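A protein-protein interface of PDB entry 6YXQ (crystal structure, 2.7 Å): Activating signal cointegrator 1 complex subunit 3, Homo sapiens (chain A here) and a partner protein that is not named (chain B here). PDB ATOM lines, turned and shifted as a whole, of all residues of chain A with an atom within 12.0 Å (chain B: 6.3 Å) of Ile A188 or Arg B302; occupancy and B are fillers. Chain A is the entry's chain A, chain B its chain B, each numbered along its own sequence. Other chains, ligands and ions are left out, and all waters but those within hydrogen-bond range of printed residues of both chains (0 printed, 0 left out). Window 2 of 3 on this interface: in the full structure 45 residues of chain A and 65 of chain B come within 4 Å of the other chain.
Among the printed residues, merely in contact across the chains: Glu A185 with Gly B310 (3.9 Å), Leu A186 with Ile B298 (3.7 Å), Leu A186 with Arg B302 (3.4 Å), Leu A186 with Leu B309 (3.8 Å), Ile A188 with Arg B302 (3.4 Å) and Asn A189 with Arg B302 (3.9 Å).
Of chain B, only Arg B302 (3.4 Å) comes within 4 Å of Ile A188.
Arg B302 touches just these residues of chain A: Leu A186 (3.4 Å), Ile A188 (3.4 Å) and Asn A189 (3.9 Å).
No residue of chain A comes within 4 Å of Leu B303.
No residue of chain A comes within 4 Å of Asp B305.
No residue of chain A comes within 4 Å of Ser B306.
Of chain A, only Leu A186 (3.8 Å) comes within 4 Å of Leu B309.
Printed residues of chain A within 4 Å of Ile B298: Leu A186 (3.7 Å).
Of the printed residues of chain B, Asn A189 touches Arg B302.
Lys B299 touches none of the printed residues of chain A.
The nearest printed residue of chain B that does not touch Ile A188 is Leu B303 (6.7 Å).
The nearest printed residue of chain A that does not touch Ile B298 is Asn A189 (7.4 Å).
Of the 7 printed residues of chain A, 4 touch a printed residue of chain B.
Printed residues of chain A that touch a printed residue of chain B: Glu A185, Leu A186, Ile A188 and Asn A189.
Hydrophobic or aromatic side chains of chain A that line the printed part of chain B: Leu A186 and Ile A188.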
ATOM      1  N   ASP A 184       0.461   1.551  26.992  1.00  0.00           N
ATOM      2  CA  ASP A 184       0.842   1.980  25.658  1.00  0.00           C
ATOM      3  C   ASP A 184       2.025   1.244  25.120  1.00  0.00           C
ATOM      4  O   ASP A 184       2.931   0.855  25.862  1.00  0.00           O
ATOM      5  CB  ASP A 184       1.223   3.434  25.549  1.00  0.00           C
ATOM      6  CG  ASP A 184       0.090   4.371  26.022  1.00  0.00           C
ATOM      7  OD1 ASP A 184      -0.819   3.960  26.701  1.00  0.00           O
ATOM      8  OD2 ASP A 184       0.193   5.484  25.697  1.00  0.00           O
ATOM      9  N   GLU A 185       1.980   1.115  23.803  1.00  0.00           N
ATOM     10  CA  GLU A 185       2.872   0.223  23.110  1.00  0.00           C
ATOM     11  C   GLU A 185       4.308   0.665  23.304  1.00  0.00           C
ATOM     12  O   GLU A 185       4.612   1.862  23.388  1.00  0.00           O
ATOM     13  CB  GLU A 185       2.471   0.177  21.641  1.00  0.00           C
ATOM     14  CG  GLU A 185       0.969  -0.044  21.492  1.00  0.00           C
ATOM     15  CD  GLU A 185       0.546  -1.465  21.843  1.00  0.00           C
ATOM     16  OE1 GLU A 185       0.376  -1.765  23.048  1.00  0.00           O
ATOM     17  OE2 GLU A 185       0.385  -2.282  20.912  1.00  0.00           O
ATOM     18  N   LEU A 186       5.152  -0.323  23.496  1.00  0.00           N
ATOM     19  CA  LEU A 186       6.584  -0.164  23.470  1.00  0.00           C
ATOM     20  C   LEU A 186       6.902   0.801  22.339  1.00  0.00           C
ATOM     21  O   LEU A 186       6.501   0.567  21.193  1.00  0.00           O
ATOM     22  CB  LEU A 186       7.246  -1.533  23.303  1.00  0.00           C
ATOM     23  CG  LEU A 186       6.657  -2.544  22.302  1.00  0.00           C
ATOM     24  CD1 LEU A 186       6.979  -2.217  20.852  1.00  0.00           C
ATOM     25  CD2 LEU A 186       7.139  -3.945  22.636  1.00  0.00           C
ATOM     26  N   PRO A 187       7.530   1.935  22.628  1.00  0.00           N
ATOM     27  CA  PRO A 187       7.791   2.905  21.559  1.00  0.00           C
ATOM     28  C   PRO A 187       8.773   2.352  20.540  1.00  0.00           C
ATOM     29  O   PRO A 187       9.323   1.260  20.719  1.00  0.00           O
ATOM     30  CB  PRO A 187       8.347   4.121  22.310  1.00  0.00           C
ATOM     31  CG  PRO A 187       8.910   3.561  23.569  1.00  0.00           C
ATOM     32  CD  PRO A 187       8.014   2.408  23.936  1.00  0.00           C
ATOM     33  N   ILE A 188       8.986   3.090  19.459  1.00  0.00           N
ATOM     34  CA  ILE A 188       9.831   2.608  18.374  1.00  0.00           C
ATOM     35  C   ILE A 188      11.295   2.747  18.774  1.00  0.00           C
ATOM     36  O   ILE A 188      11.734   3.810  19.236  1.00  0.00           O
ATOM     37  CB  ILE A 188       9.520   3.357  17.070  1.00  0.00           C
ATOM     38  CG1 ILE A 188       8.005   3.427  16.855  1.00  0.00           C
ATOM     39  CG2 ILE A 188      10.193   2.668  15.895  1.00  0.00           C
ATOM     40  CD1 ILE A 188       7.365   2.089  16.523  1.00  0.00           C
ATOM     41  N   ASN A 189      12.054   1.671  18.582  1.00  0.00           N
ATOM     42  CA  ASN A 189      13.399   1.518  19.116  1.00  0.00           C
ATOM     43  C   ASN A 189      14.449   2.041  18.140  1.00  0.00           C
ATOM     44  O   ASN A 189      14.277   1.984  16.919  1.00  0.00           O
ATOM     45  CB  ASN A 189      13.673   0.043  19.426  1.00  0.00           C
ATOM     46  CG  ASN A 189      14.141  -0.185  20.852  1.00  0.00           C
ATOM     47  OD1 ASN A 189      13.558   0.341  21.801  1.00  0.00           O
ATOM     48  ND2 ASN A 189      15.190  -0.985  21.010  1.00  0.00           N
ATOM     49  N   GLY A 190      15.550   2.544  18.696  1.00  0.00           N
ATOM     50  CA  GLY A 190      16.666   3.021  17.898  1.00  0.00           C
ATOM     51  C   GLY A 190      17.177   4.392  18.299  1.00  0.00           C
ATOM     52  O   GLY A 190      17.995   4.524  19.211  1.00  0.00           O
ATOM     53  N   ALA B 297      13.907  -6.938  27.576  1.00  0.00           N
ATOM     54  CA  ALA B 297      13.816  -8.032  26.616  1.00  0.00           C
ATOM     55  C   ALA B 297      12.651  -7.834  25.656  1.00  0.00           C
ATOM     56  O   ALA B 297      12.800  -8.031  24.440  1.00  0.00           O
ATOM     57  CB  ALA B 297      13.686  -9.362  27.349  1.00  0.00           C
ATOM     58  N   ILE B 298      11.483  -7.452  26.184  1.00  0.00           N
ATOM     59  CA  ILE B 298      10.322  -7.201  25.336  1.00  0.00           C
ATOM     60  C   ILE B 298      10.630  -6.087  24.345  1.00  0.00           C
ATOM     61  O   ILE B 298      10.351  -6.198  23.140  1.00  0.00           O
ATOM     62  CB  ILE B 298       9.093  -6.869  26.201  1.00  0.00           C
ATOM     63  CG1 ILE B 298       8.575  -8.124  26.902  1.00  0.00           C
ATOM     64  CG2 ILE B 298       7.997  -6.266  25.362  1.00  0.00           C
ATOM     65  CD1 ILE B 298       7.300  -7.897  27.662  1.00  0.00           C
ATOM     66  N   LYS B 299      11.246  -5.007  24.833  1.00  0.00           N
ATOM     67  CA  LYS B 299      11.577  -3.892  23.955  1.00  0.00           C
ATOM     68  C   LYS B 299      12.537  -4.326  22.855  1.00  0.00           C
ATOM     69  O   LYS B 299      12.317  -4.034  21.673  1.00  0.00           O
ATOM     70  CB  LYS B 299      12.165  -2.742  24.773  1.00  0.00           C
ATOM     71  CG  LYS B 299      11.116  -1.972  25.559  1.00  0.00           C
ATOM     72  CD  LYS B 299      11.577  -0.570  25.894  1.00  0.00           C
ATOM     73  CE  LYS B 299      12.492  -0.559  27.101  1.00  0.00           C
ATOM     74  NZ  LYS B 299      12.129   0.541  28.042  1.00  0.00           N
ATOM     75  N   LYS B 300      13.602  -5.044  23.227  1.00  0.00           N
ATOM     76  CA  LYS B 300      14.612  -5.454  22.256  1.00  0.00           C
ATOM     77  C   LYS B 300      14.016  -6.357  21.187  1.00  0.00           C
ATOM     78  O   LYS B 300      14.271  -6.173  19.991  1.00  0.00           O
ATOM     79  CB  LYS B 300      15.765  -6.168  22.964  1.00  0.00           C
ATOM     80  CG  LYS B 300      16.927  -5.274  23.357  1.00  0.00           C
ATOM     81  CD  LYS B 300      17.565  -5.740  24.661  1.00  0.00           C
ATOM     82  CE  LYS B 300      17.833  -7.238  24.654  1.00  0.00           C
ATOM     83  NZ  LYS B 300      18.462  -7.687  25.926  1.00  0.00           N
ATOM     84  N   ARG B 301      13.215  -7.340  21.596  1.00  0.00           N
ATOM     85  CA  ARG B 301      12.724  -8.357  20.676  1.00  0.00           C
ATOM     86  C   ARG B 301      11.359  -8.024  20.076  1.00  0.00           C
ATOM     87  O   ARG B 301      10.723  -8.914  19.502  1.00  0.00           O
ATOM     88  CB  ARG B 301      12.671  -9.713  21.388  1.00  0.00           C
ATOM     89  CG  ARG B 301      13.963 -10.081  22.110  1.00  0.00           C
ATOM     90  CD  ARG B 301      13.797 -11.293  23.016  1.00  0.00           C
ATOM     91  NE  ARG B 301      13.254 -12.449  22.307  1.00  0.00           N
ATOM     92  CZ  ARG B 301      13.277 -13.693  22.775  1.00  0.00           C
ATOM     93  NH1 ARG B 301      13.827 -13.955  23.952  1.00  0.00           N
ATOM     94  NH2 ARG B 301      12.753 -14.679  22.062  1.00  0.00           N
ATOM     95  N   ARG B 302      10.885  -6.779  20.219  1.00  0.00           N
ATOM     96  CA  ARG B 302       9.598  -6.386  19.637  1.00  0.00           C
ATOM     97  C   ARG B 302       9.428  -6.769  18.164  1.00  0.00           C
ATOM     98  O   ARG B 302       8.310  -7.091  17.740  1.00  0.00           O
ATOM     99  CB  ARG B 302       9.388  -4.877  19.810  1.00  0.00           C
ATOM    100  CG  ARG B 302      10.271  -3.982  18.951  1.00  0.00           C
ATOM    101  CD  ARG B 302       9.914  -2.516  19.162  1.00  0.00           C
ATOM    102  NE  ARG B 302      10.165  -1.699  17.978  1.00  0.00           N
ATOM    103  CZ  ARG B 302       9.271  -1.474  17.019  1.00  0.00           C
ATOM    104  NH1 ARG B 302       9.592  -0.713  15.980  1.00  0.00           N
ATOM    105  NH2 ARG B 302       8.059  -2.012  17.095  1.00  0.00           N
ATOM    106  N   LEU B 303      10.498  -6.735  17.361  1.00  0.00           N
ATOM    107  CA  LEU B 303      10.305  -6.951  15.925  1.00  0.00           C
ATOM    108  C   LEU B 303      10.360  -8.420  15.526  1.00  0.00           C
ATOM    109  O   LEU B 303      10.018  -8.746  14.382  1.00  0.00           O
ATOM    110  CB  LEU B 303      11.324  -6.142  15.104  1.00  0.00           C
ATOM    111  CG  LEU B 303      11.360  -4.646  15.432  1.00  0.00           C
ATOM    112  CD1 LEU B 303      12.750  -4.061  15.227  1.00  0.00           C
ATOM    113  CD2 LEU B 303      10.306  -3.866  14.641  1.00  0.00           C
ATOM    114  N   GLU B 304      10.777  -9.306  16.433  1.00  0.00           N
ATOM    115  CA  GLU B 304      10.559 -10.731  16.213  1.00  0.00           C
ATOM    116  C   GLU B 304       9.077 -11.016  16.004  1.00  0.00           C
ATOM    117  O   GLU B 304       8.703 -11.812  15.133  1.00  0.00           O
ATOM    118  CB  GLU B 304      11.098 -11.543  17.392  1.00  0.00           C
ATOM    119  CG  GLU B 304      12.590 -11.379  17.651  1.00  0.00           C
ATOM    120  CD  GLU B 304      13.121 -12.361  18.689  1.00  0.00           C
ATOM    121  OE1 GLU B 304      14.332 -12.294  19.011  1.00  0.00           O
ATOM    122  OE2 GLU B 304      12.327 -13.199  19.180  1.00  0.00           O
ATOM    123  N   ASP B 305       8.218 -10.360  16.788  1.00  0.00           N
ATOM    124  CA  ASP B 305       6.773 -10.441  16.584  1.00  0.00           C
ATOM    125  C   ASP B 305       6.147  -9.127  17.059  1.00  0.00           C
ATOM    126  O   ASP B 305       5.767  -8.991  18.223  1.00  0.00           O
ATOM    127  CB  ASP B 305       6.167 -11.638  17.295  1.00  0.00           C
ATOM    128  CG  ASP B 305       4.817 -12.016  16.733  1.00  0.00           C
ATOM    129  OD1 ASP B 305       4.052 -11.103  16.351  1.00  0.00           O
ATOM    130  OD2 ASP B 305       4.521 -13.224  16.675  1.00  0.00           O
ATOM    131  N   SER B 306       6.106  -8.155  16.150  1.00  0.00           N
ATOM    132  CA  SER B 306       5.222  -6.991  16.186  1.00  0.00           C
ATOM    133  C   SER B 306       4.049  -7.098  17.159  1.00  0.00           C
ATOM    134  O   SER B 306       3.999  -6.365  18.155  1.00  0.00           O
ATOM    135  CB  SER B 306       4.686  -6.736  14.774  1.00  0.00           C
ATOM    136  OG  SER B 306       3.614  -5.809  14.768  1.00  0.00           O
ATOM    137  N   LYS B 307       3.110  -8.011  16.891  1.00  0.00           N
ATOM    138  CA  LYS B 307       1.844  -8.011  17.623  1.00  0.00           C
ATOM    139  C   LYS B 307       1.956  -8.722  18.965  1.00  0.00           C
ATOM    140  O   LYS B 307       1.366  -8.274  19.959  1.00  0.00           O
ATOM    141  CB  LYS B 307       0.745  -8.664  16.780  1.00  0.00           C
ATOM    142  CG  LYS B 307      -0.180  -7.684  16.056  1.00  0.00           C
ATOM    143  CD  LYS B 307       0.593  -6.499  15.484  1.00  0.00           C
ATOM    144  CE  LYS B 307      -0.278  -5.256  15.362  1.00  0.00           C
ATOM    145  NZ  LYS B 307       0.536  -4.010  15.294  1.00  0.00           N
ATOM    146  N   LEU B 309       4.639  -9.073  20.934  1.00  0.00           N
ATOM    147  CA  LEU B 309       5.437  -8.343  21.911  1.00  0.00           C
ATOM    148  C   LEU B 309       4.700  -7.128  22.457  1.00  0.00           C
ATOM    149  O   LEU B 309       4.866  -6.785  23.633  1.00  0.00           O
ATOM    150  CB  LEU B 309       6.768  -7.927  21.292  1.00  0.00           C
ATOM    151  CG  LEU B 309       7.925  -8.918  21.459  1.00  0.00           C
ATOM    152  CD1 LEU B 309       8.163  -9.215  22.922  1.00  0.00           C
ATOM    153  CD2 LEU B 309       7.694 -10.203  20.683  1.00  0.00           C
ATOM    154  N   GLY B 310       3.865  -6.481  21.642  1.00  0.00           N
ATOM    155  CA  GLY B 310       3.042  -5.396  22.156  1.00  0.00           C
ATOM    156  C   GLY B 310       1.998  -5.874  23.151  1.00  0.00           C
ATOM    157  O   GLY B 310       1.737  -5.209  24.161  1.00  0.00           O
